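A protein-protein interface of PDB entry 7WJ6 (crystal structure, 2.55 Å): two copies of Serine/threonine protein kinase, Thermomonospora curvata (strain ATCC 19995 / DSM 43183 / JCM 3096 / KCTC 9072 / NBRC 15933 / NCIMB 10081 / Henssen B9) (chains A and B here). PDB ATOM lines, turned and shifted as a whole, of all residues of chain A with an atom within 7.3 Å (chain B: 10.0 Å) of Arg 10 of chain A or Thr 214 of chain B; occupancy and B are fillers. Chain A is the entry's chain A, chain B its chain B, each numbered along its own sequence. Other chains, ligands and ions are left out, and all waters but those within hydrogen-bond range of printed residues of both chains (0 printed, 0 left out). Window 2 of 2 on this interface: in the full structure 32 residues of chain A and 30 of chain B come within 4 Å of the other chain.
The backbone NH (N) of Ile 11 of chain A sits at hydrogen-bond distance from the side-chain hydroxyl (OG1) of Thr 214 of chain B.
NH2 of Arg 10 of chain A lies within salt-bridge range of OE2 of Glu 12 of chain A (3.8 Å). N of Arg 10 of chain A lies within hydrogen-bond range of O of Ile 27 of chain A, 3.0 Å away. N of Glu 12 of chain A sits at hydrogen-bond distance from O of Ala 25 of chain A (2.9 Å). The backbone carbonyl oxygen (O) of Ala 13 of chain A sits at hydrogen-bond distance from the backbone NH (N) of Ala 25 of chain A (3.1 Å).
Among the printed residues, pairs that only touch across the chains: Glu 12 of chain A with Ala 103 of chain B, Ala 13 of chain A with Leu 213 of chain B, Leu 7 of chain A with Val 218 of chain B, Tyr 9 of chain A with Thr 214 of chain B, Arg 10 of chain A with Thr 214 of chain B, Ile 11 of chain A with Leu 213 of chain B and Ile 11 of chain A with Leu 217 of chain B.
Ile 11 of chain A touches three residues of chain B. Of the printed residues of chain B, Glu 12 of chain A touches Ala 103 (3.2 Å). No residue of chain B comes within 4 Å of Gly 26 of chain A. Ala 185 of chain B touches none of the printed residues of chain A. Thr 214 of chain B touches just these residues of chain A: Tyr 9, Arg 10 and Ile 11. Of the printed residues of chain A, Leu 217 of chain B touches Ile 11. The nearest residue of chain B that does not touch Arg 10 of chain A is Leu 213 of chain B (6.9 Å). The nearest residue of chain A that does not touch Thr 214 of chain B is Leu 7 of chain A (5.0 Å).
Hydrophobic or aromatic side chains of chain A within 4 Å of the printed part of chain B: Leu 7 and Ile 11. Among the printed residues, 8 pairs touch across the chains.
No position is printed for both chains. Of the 8 pairs that touch across the chains among the printed residues, none has its exchanged pair printed and touching as well.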
ATOM      1  N   LEU A   7      13.122  11.241  11.235  1.00  0.00           N
ATOM      2  CA  LEU A   7      13.665  12.116  10.204  1.00  0.00           C
ATOM      3  C   LEU A   7      14.957  11.573   9.612  1.00  0.00           C
ATOM      4  O   LEU A   7      15.871  11.191  10.345  1.00  0.00           O
ATOM      5  CB  LEU A   7      13.908  13.521  10.753  1.00  0.00           C
ATOM      6  CG  LEU A   7      12.757  14.523  10.650  1.00  0.00           C
ATOM      7  CD1 LEU A   7      13.309  15.939  10.578  1.00  0.00           C
ATOM      8  CD2 LEU A   7      11.871  14.219   9.448  1.00  0.00           C
ATOM      9  N   PRO A   8      15.033  11.540   8.278  1.00  0.00           N
ATOM     10  CA  PRO A   8      16.287  11.157   7.614  1.00  0.00           C
ATOM     11  C   PRO A   8      17.361  12.230   7.652  1.00  0.00           C
ATOM     12  O   PRO A   8      18.447  12.012   7.104  1.00  0.00           O
ATOM     13  CB  PRO A   8      15.847  10.889   6.164  1.00  0.00           C
ATOM     14  CG  PRO A   8      14.341  10.889   6.182  1.00  0.00           C
ATOM     15  CD  PRO A   8      13.951  11.773   7.314  1.00  0.00           C
ATOM     16  N   TYR A   9      17.093  13.376   8.269  1.00  0.00           N
ATOM     17  CA  TYR A   9      18.019  14.496   8.296  1.00  0.00           C
ATOM     18  C   TYR A   9      18.455  14.782   9.724  1.00  0.00           C
ATOM     19  O   TYR A   9      17.682  14.621  10.673  1.00  0.00           O
ATOM     20  CB  TYR A   9      17.384  15.751   7.680  1.00  0.00           C
ATOM     21  CG  TYR A   9      16.798  15.515   6.308  1.00  0.00           C
ATOM     22  CD1 TYR A   9      17.609  15.496   5.182  1.00  0.00           C
ATOM     23  CD2 TYR A   9      15.438  15.294   6.139  1.00  0.00           C
ATOM     24  CE1 TYR A   9      17.084  15.274   3.925  1.00  0.00           C
ATOM     25  CE2 TYR A   9      14.902  15.071   4.880  1.00  0.00           C
ATOM     26  CZ  TYR A   9      15.733  15.061   3.779  1.00  0.00           C
ATOM     27  OH  TYR A   9      15.217  14.840   2.525  1.00  0.00           O
ATOM     28  N   ARG A  10      19.705  15.211   9.868  1.00  0.00           N
ATOM     29  CA  ARG A  10      20.234  15.661  11.147  1.00  0.00           C
ATOM     30  C   ARG A  10      20.662  17.113  11.010  1.00  0.00           C
ATOM     31  O   ARG A  10      21.471  17.447  10.137  1.00  0.00           O
ATOM     32  CB  ARG A  10      21.413  14.802  11.607  1.00  0.00           C
ATOM     33  CG  ARG A  10      21.992  15.257  12.942  1.00  0.00           C
ATOM     34  CD  ARG A  10      23.229  14.467  13.326  1.00  0.00           C
ATOM     35  NE  ARG A  10      24.256  14.519  12.295  1.00  0.00           N
ATOM     36  CZ  ARG A  10      24.727  13.455  11.660  1.00  0.00           C
ATOM     37  NH1 ARG A  10      24.279  12.239  11.926  1.00  0.00           N
ATOM     38  NH2 ARG A  10      25.671  13.615  10.737  1.00  0.00           N
ATOM     39  N   ILE A  11      20.128  17.968  11.877  1.00  0.00           N
ATOM     40  CA  ILE A  11      20.410  19.396  11.819  1.00  0.00           C
ATOM     41  C   ILE A  11      21.725  19.671  12.530  1.00  0.00           C
ATOM     42  O   ILE A  11      21.944  19.213  13.656  1.00  0.00           O
ATOM     43  CB  ILE A  11      19.267  20.210  12.450  1.00  0.00           C
ATOM     44  CG1 ILE A  11      17.887  19.697  12.017  1.00  0.00           C
ATOM     45  CG2 ILE A  11      19.419  21.671  12.097  1.00  0.00           C
ATOM     46  CD1 ILE A  11      17.727  19.475  10.535  1.00  0.00           C
ATOM     47  N   GLU A  12      22.608  20.426  11.874  1.00  0.00           N
ATOM     48  CA  GLU A  12      23.927  20.708  12.418  1.00  0.00           C
ATOM     49  C   GLU A  12      24.141  22.171  12.769  1.00  0.00           C
ATOM     50  O   GLU A  12      25.038  22.471  13.563  1.00  0.00           O
ATOM     51  CB  GLU A  12      25.021  20.275  11.428  1.00  0.00           C
ATOM     52  CG  GLU A  12      24.981  18.800  11.067  1.00  0.00           C
ATOM     53  CD  GLU A  12      26.171  18.373  10.229  1.00  0.00           C
ATOM     54  OE1 GLU A  12      26.592  19.154   9.349  1.00  0.00           O
ATOM     55  OE2 GLU A  12      26.683  17.254  10.445  1.00  0.00           O
ATOM     56  N   ALA A  13      23.352  23.084  12.205  1.00  0.00           N
ATOM     57  CA  ALA A  13      23.516  24.501  12.480  1.00  0.00           C
ATOM     58  C   ALA A  13      22.199  25.227  12.250  1.00  0.00           C
ATOM     59  O   ALA A  13      21.378  24.818  11.426  1.00  0.00           O
ATOM     60  CB  ALA A  13      24.620  25.118  11.616  1.00  0.00           C
ATOM     61  N   ALA A  25      21.066  24.313   8.414  1.00  0.00           N
ATOM     62  CA  ALA A  25      21.979  23.493   7.635  1.00  0.00           C
ATOM     63  C   ALA A  25      21.980  22.088   8.215  1.00  0.00           C
ATOM     64  O   ALA A  25      22.078  21.915   9.434  1.00  0.00           O
ATOM     65  CB  ALA A  25      23.392  24.074   7.646  1.00  0.00           C
ATOM     66  N   GLY A  26      21.870  21.092   7.349  1.00  0.00           N
ATOM     67  CA  GLY A  26      21.802  19.732   7.830  1.00  0.00           C
ATOM     68  C   GLY A  26      22.496  18.736   6.933  1.00  0.00           C
ATOM     69  O   GLY A  26      23.204  19.106   5.990  1.00  0.00           O
ATOM     70  N   ILE A  27      22.298  17.458   7.227  1.00  0.00           N
ATOM     71  CA  ILE A  27      22.902  16.377   6.465  1.00  0.00           C
ATOM     72  C   ILE A  27      21.856  15.287   6.300  1.00  0.00           C
ATOM     73  O   ILE A  27      21.191  14.905   7.269  1.00  0.00           O
ATOM     74  CB  ILE A  27      24.171  15.834   7.154  1.00  0.00           C
ATOM     75  CG1 ILE A  27      25.396  16.626   6.696  1.00  0.00           C
ATOM     76  CG2 ILE A  27      24.357  14.348   6.871  1.00  0.00           C
ATOM     77  CD1 ILE A  27      26.693  16.173   7.327  1.00  0.00           C
ATOM     78  N   ASP A  28      21.687  14.811   5.071  1.00  0.00           N
ATOM     79  CA  ASP A  28      20.914  13.600   4.831  1.00  0.00           C
ATOM     80  C   ASP A  28      21.701  12.417   5.377  1.00  0.00           C
ATOM     81  O   ASP A  28      22.781  12.096   4.868  1.00  0.00           O
ATOM     82  CB  ASP A  28      20.629  13.444   3.339  1.00  0.00           C
ATOM     83  CG  ASP A  28      19.496  12.472   3.054  1.00  0.00           C
ATOM     84  OD1 ASP A  28      19.311  11.509   3.828  1.00  0.00           O
ATOM     85  OD2 ASP A  28      18.779  12.678   2.053  1.00  0.00           O
ATOM     86  N   THR A  29      21.182  11.778   6.427  1.00  0.00           N
ATOM     87  CA  THR A  29      21.909  10.671   7.040  1.00  0.00           C
ATOM     88  C   THR A  29      22.007   9.466   6.115  1.00  0.00           C
ATOM     89  O   THR A  29      22.906   8.636   6.291  1.00  0.00           O
ATOM     90  CB  THR A  29      21.246  10.260   8.358  1.00  0.00           C
ATOM     91  OG1 THR A  29      20.048   9.523   8.084  1.00  0.00           O
ATOM     92  CG2 THR A  29      20.905  11.488   9.193  1.00  0.00           C
ATOM     93  N   GLY A  32      24.811  11.377   3.452  1.00  0.00           N
ATOM     94  CA  GLY A  32      25.832  12.330   3.837  1.00  0.00           C
ATOM     95  C   GLY A  32      25.820  13.630   3.066  1.00  0.00           C
ATOM     96  O   GLY A  32      26.722  14.452   3.261  1.00  0.00           O
ATOM     97  N   VAL A  35      22.588  19.585   3.036  1.00  0.00           N
ATOM     98  CA  VAL A  35      21.276  20.104   2.678  1.00  0.00           C
ATOM     99  C   VAL A  35      20.997  21.380   3.458  1.00  0.00           C
ATOM    100  O   VAL A  35      21.664  21.700   4.445  1.00  0.00           O
ATOM    101  CB  VAL A  35      20.146  19.083   2.930  1.00  0.00           C
ATOM    102  CG1 VAL A  35      20.416  17.794   2.187  1.00  0.00           C
ATOM    103  CG2 VAL A  35      19.988  18.827   4.420  1.00  0.00           C
ATOM    104  N   LEU A  37      17.592  23.153   5.279  1.00  0.00           N
ATOM    105  CA  LEU A  37      16.236  22.867   5.728  1.00  0.00           C
ATOM    106  C   LEU A  37      15.548  24.166   6.108  1.00  0.00           C
ATOM    107  O   LEU A  37      16.026  24.892   6.986  1.00  0.00           O
ATOM    108  CB  LEU A  37      16.239  21.884   6.895  1.00  0.00           C
ATOM    109  CG  LEU A  37      15.849  20.490   6.406  1.00  0.00           C
ATOM    110  CD1 LEU A  37      16.191  19.418   7.418  1.00  0.00           C
ATOM    111  CD2 LEU A  37      14.367  20.469   6.083  1.00  0.00           C
ATOM    112  N   PHE A  87       8.231  21.383   6.044  1.00  0.00           N
ATOM    113  CA  PHE A  87       9.675  21.382   5.850  1.00  0.00           C
ATOM    114  C   PHE A  87      10.007  21.410   4.365  1.00  0.00           C
ATOM    115  O   PHE A  87       9.338  20.757   3.558  1.00  0.00           O
ATOM    116  CB  PHE A  87      10.326  20.161   6.503  1.00  0.00           C
ATOM    117  CG  PHE A  87      10.193  20.135   7.996  1.00  0.00           C
ATOM    118  CD1 PHE A  87       9.050  19.629   8.595  1.00  0.00           C
ATOM    119  CD2 PHE A  87      11.208  20.621   8.800  1.00  0.00           C
ATOM    120  CE1 PHE A  87       8.923  19.607   9.966  1.00  0.00           C
ATOM    121  CE2 PHE A  87      11.085  20.599  10.172  1.00  0.00           C
ATOM    122  CZ  PHE A  87       9.941  20.092  10.756  1.00  0.00           C
ATOM    123  N   PHE B 102      24.712  26.271  19.056  1.00  0.00           N
ATOM    124  CA  PHE B 102      24.028  24.998  18.861  1.00  0.00           C
ATOM    125  C   PHE B 102      24.723  24.104  17.843  1.00  0.00           C
ATOM    126  O   PHE B 102      24.305  22.955  17.670  1.00  0.00           O
ATOM    127  CB  PHE B 102      22.574  25.237  18.441  1.00  0.00           C
ATOM    128  N   ALA B 103      25.759  24.594  17.168  1.00  0.00           N
ATOM    129  CA  ALA B 103      26.464  23.800  16.173  1.00  0.00           C
ATOM    130  C   ALA B 103      27.669  23.063  16.736  1.00  0.00           C
ATOM    131  O   ALA B 103      28.192  22.164  16.067  1.00  0.00           O
ATOM    132  CB  ALA B 103      26.914  24.692  15.010  1.00  0.00           C
ATOM    133  N   MET B 151      16.718  32.392  20.139  1.00  0.00           N
ATOM    134  CA  MET B 151      18.167  32.210  20.110  1.00  0.00           C
ATOM    135  C   MET B 151      18.851  33.019  19.018  1.00  0.00           C
ATOM    136  O   MET B 151      20.062  33.239  19.101  1.00  0.00           O
ATOM    137  CB  MET B 151      18.524  30.736  19.927  1.00  0.00           C
ATOM    138  CG  MET B 151      17.836  30.071  18.750  1.00  0.00           C
ATOM    139  SD  MET B 151      18.515  28.438  18.383  1.00  0.00           S
ATOM    140  CE  MET B 151      17.006  27.525  18.048  1.00  0.00           C
ATOM    141  N   PRO B 184      11.111  29.671  17.183  1.00  0.00           N
ATOM    142  CA  PRO B 184      11.695  28.623  16.330  1.00  0.00           C
ATOM    143  C   PRO B 184      11.474  27.216  16.856  1.00  0.00           C
ATOM    144  O   PRO B 184      11.501  26.265  16.064  1.00  0.00           O
ATOM    145  CB  PRO B 184      13.189  28.980  16.295  1.00  0.00           C
ATOM    146  CG  PRO B 184      13.404  29.922  17.430  1.00  0.00           C
ATOM    147  CD  PRO B 184      12.114  30.656  17.614  1.00  0.00           C
ATOM    148  N   ALA B 185      11.251  27.052  18.159  1.00  0.00           N
ATOM    149  CA  ALA B 185      11.115  25.740  18.781  1.00  0.00           C
ATOM    150  C   ALA B 185       9.669  25.280  18.929  1.00  0.00           C
ATOM    151  O   ALA B 185       9.389  24.089  18.765  1.00  0.00           O
ATOM    152  CB  ALA B 185      11.786  25.739  20.159  1.00  0.00           C
ATOM    153  N   ALA B 208      14.912  24.923  25.180  1.00  0.00           N
ATOM    154  CA  ALA B 208      15.715  24.945  23.960  1.00  0.00           C
ATOM    155  C   ALA B 208      17.207  24.942  24.251  1.00  0.00           C
ATOM    156  O   ALA B 208      17.989  24.409  23.458  1.00  0.00           O
ATOM    157  CB  ALA B 208      15.347  26.163  23.112  1.00  0.00           C
ATOM    158  N   PHE B 210      18.811  23.150  26.098  1.00  0.00           N
ATOM    159  CA  PHE B 210      19.297  21.801  26.330  1.00  0.00           C
ATOM    160  C   PHE B 210      18.874  20.802  25.264  1.00  0.00           C
ATOM    161  O   PHE B 210      19.353  19.663  25.289  1.00  0.00           O
ATOM    162  CB  PHE B 210      18.823  21.290  27.699  1.00  0.00           C
ATOM    163  CG  PHE B 210      19.267  22.140  28.851  1.00  0.00           C
ATOM    164  CD1 PHE B 210      20.557  22.039  29.349  1.00  0.00           C
ATOM    165  CD2 PHE B 210      18.395  23.041  29.438  1.00  0.00           C
ATOM    166  CE1 PHE B 210      20.970  22.824  30.413  1.00  0.00           C
ATOM    167  CE2 PHE B 210      18.800  23.828  30.502  1.00  0.00           C
ATOM    168  CZ  PHE B 210      20.089  23.719  30.990  1.00  0.00           C
ATOM    169  N   LEU B 211      18.020  21.179  24.349  1.00  0.00           N
ATOM    170  CA  LEU B 211      17.629  20.174  23.374  1.00  0.00           C
ATOM    171  C   LEU B 211      18.538  20.224  22.151  1.00  0.00           C
ATOM    172  O   LEU B 211      19.046  21.291  21.785  1.00  0.00           O
ATOM    173  CB  LEU B 211      16.183  20.388  22.942  1.00  0.00           C
ATOM    174  CG  LEU B 211      15.144  20.210  24.047  1.00  0.00           C
ATOM    175  CD1 LEU B 211      13.745  20.328  23.484  1.00  0.00           C
ATOM    176  CD2 LEU B 211      15.336  18.871  24.728  1.00  0.00           C
ATOM    177  N   PRO B 212      18.771  19.074  21.521  1.00  0.00           N
ATOM    178  CA  PRO B 212      19.490  19.072  20.244  1.00  0.00           C
ATOM    179  C   PRO B 212      18.670  19.762  19.167  1.00  0.00           C
ATOM    180  O   PRO B 212      17.435  19.763  19.197  1.00  0.00           O
ATOM    181  CB  PRO B 212      19.673  17.580  19.934  1.00  0.00           C
ATOM    182  CG  PRO B 212      19.370  16.861  21.216  1.00  0.00           C
ATOM    183  CD  PRO B 212      18.385  17.718  21.942  1.00  0.00           C
ATOM    184  N   LEU B 213      19.381  20.357  18.206  1.00  0.00           N
ATOM    185  CA  LEU B 213      18.716  21.140  17.168  1.00  0.00           C
ATOM    186  C   LEU B 213      17.656  20.311  16.456  1.00  0.00           C
ATOM    187  O   LEU B 213      16.538  20.788  16.225  1.00  0.00           O
ATOM    188  CB  LEU B 213      19.750  21.667  16.175  1.00  0.00           C
ATOM    189  CG  LEU B 213      20.213  23.109  16.379  1.00  0.00           C
ATOM    190  CD1 LEU B 213      20.837  23.657  15.106  1.00  0.00           C
ATOM    191  CD2 LEU B 213      19.055  23.986  16.838  1.00  0.00           C
ATOM    192  N   THR B 214      17.979  19.056  16.134  1.00  0.00           N
ATOM    193  CA  THR B 214      17.028  18.187  15.448  1.00  0.00           C
ATOM    194  C   THR B 214      15.788  17.953  16.302  1.00  0.00           C
ATOM    195  O   THR B 214      14.655  18.060  15.819  1.00  0.00           O
ATOM    196  CB  THR B 214      17.696  16.856  15.100  1.00  0.00           C
ATOM    197  OG1 THR B 214      18.977  17.101  14.500  1.00  0.00           O
ATOM    198  CG2 THR B 214      16.828  16.064  14.139  1.00  0.00           C
ATOM    199  N   THR B 215      15.988  17.627  17.582  1.00  0.00           N
ATOM    200  CA  THR B 215      14.861  17.457  18.492  1.00  0.00           C
ATOM    201  C   THR B 215      14.083  18.756  18.653  1.00  0.00           C
ATOM    202  O   THR B 215      12.851  18.746  18.755  1.00  0.00           O
ATOM    203  CB  THR B 215      15.354  16.964  19.852  1.00  0.00           C
ATOM    204  OG1 THR B 215      16.215  15.834  19.670  1.00  0.00           O
ATOM    205  CG2 THR B 215      14.179  16.570  20.734  1.00  0.00           C
ATOM    206  N   LEU B 216      14.794  19.886  18.684  1.00  0.00           N
ATOM    207  CA  LEU B 216      14.144  21.179  18.868  1.00  0.00           C
ATOM    208  C   LEU B 216      13.098  21.441  17.790  1.00  0.00           C
ATOM    209  O   LEU B 216      12.000  21.925  18.085  1.00  0.00           O
ATOM    210  CB  LEU B 216      15.196  22.286  18.887  1.00  0.00           C
ATOM    211  CG  LEU B 216      14.863  23.513  19.731  1.00  0.00           C
ATOM    212  CD1 LEU B 216      14.270  23.083  21.058  1.00  0.00           C
ATOM    213  CD2 LEU B 216      16.112  24.347  19.950  1.00  0.00           C
ATOM    214  N   LEU B 217      13.421  21.129  16.534  1.00  0.00           N
ATOM    215  CA  LEU B 217      12.513  21.430  15.432  1.00  0.00           C
ATOM    216  C   LEU B 217      11.358  20.434  15.338  1.00  0.00           C
ATOM    217  O   LEU B 217      10.228  20.820  15.020  1.00  0.00           O
ATOM    218  CB  LEU B 217      13.287  21.463  14.116  1.00  0.00           C
ATOM    219  CG  LEU B 217      14.283  22.610  13.966  1.00  0.00           C
ATOM    220  CD1 LEU B 217      15.142  22.411  12.727  1.00  0.00           C
ATOM    221  CD2 LEU B 217      13.551  23.939  13.915  1.00  0.00           C
ATOM    222  N   VAL B 218      11.619  19.154  15.599  1.00  0.00           N
ATOM    223  CA  VAL B 218      10.620  18.120  15.333  1.00  0.00           C
ATOM    224  C   VAL B 218       9.535  18.095  16.408  1.00  0.00           C
ATOM    225  O   VAL B 218       8.351  17.913  16.104  1.00  0.00           O
ATOM    226  CB  VAL B 218      11.313  16.753  15.191  1.00  0.00           C
ATOM    227  CG1 VAL B 218      10.301  15.620  15.279  1.00  0.00           C
ATOM    228  CG2 VAL B 218      12.075  16.689  13.884  1.00  0.00           C
ATOM    229  N   GLN B 219       9.906  18.291  17.670  1.00  0.00           N
ATOM    230  CA  GLN B 219       8.978  18.061  18.768  1.00  0.00           C
ATOM    231  C   GLN B 219       7.990  19.213  18.914  1.00  0.00           C
ATOM    232  O   GLN B 219       8.361  20.388  18.843  1.00  0.00           O
ATOM    233  CB  GLN B 219       9.744  17.858  20.075  1.00  0.00           C
ATOM    234  CG  GLN B 219      10.523  16.557  20.124  1.00  0.00           C
ATOM    235  CD  GLN B 219       9.751  15.391  19.531  1.00  0.00           C
ATOM    236  OE1 GLN B 219       8.665  15.046  20.000  1.00  0.00           O
ATOM    237  NE2 GLN B 219      10.311  14.776  18.496  1.00  0.00           N
ATOM    238  N   ASP B 220       6.728  18.858  19.136  1.00  0.00           N
ATOM    239  CA  ASP B 220       5.638  19.815  19.205  1.00  0.00           C
ATOM    240  C   ASP B 220       5.433  20.292  20.640  1.00  0.00           C
ATOM    241  O   ASP B 220       6.014  19.767  21.592  1.00  0.00           O
ATOM    242  CB  ASP B 220       4.347  19.196  18.664  1.00  0.00           C
ATOM    243  N   LEU B 227       9.529  16.392  27.281  1.00  0.00           N
ATOM    244  CA  LEU B 227      10.843  16.956  26.996  1.00  0.00           C
ATOM    245  C   LEU B 227      11.537  17.419  28.272  1.00  0.00           C
ATOM    246  O   LEU B 227      12.730  17.160  28.462  1.00  0.00           O
ATOM    247  CB  LEU B 227      10.717  18.108  26.000  1.00  0.00           C
ATOM    248  CG  LEU B 227      10.427  17.677  24.563  1.00  0.00           C
ATOM    249  CD1 LEU B 227      10.443  18.873  23.627  1.00  0.00           C
ATOM    250  CD2 LEU B 227      11.432  16.627  24.115  1.00  0.00           C
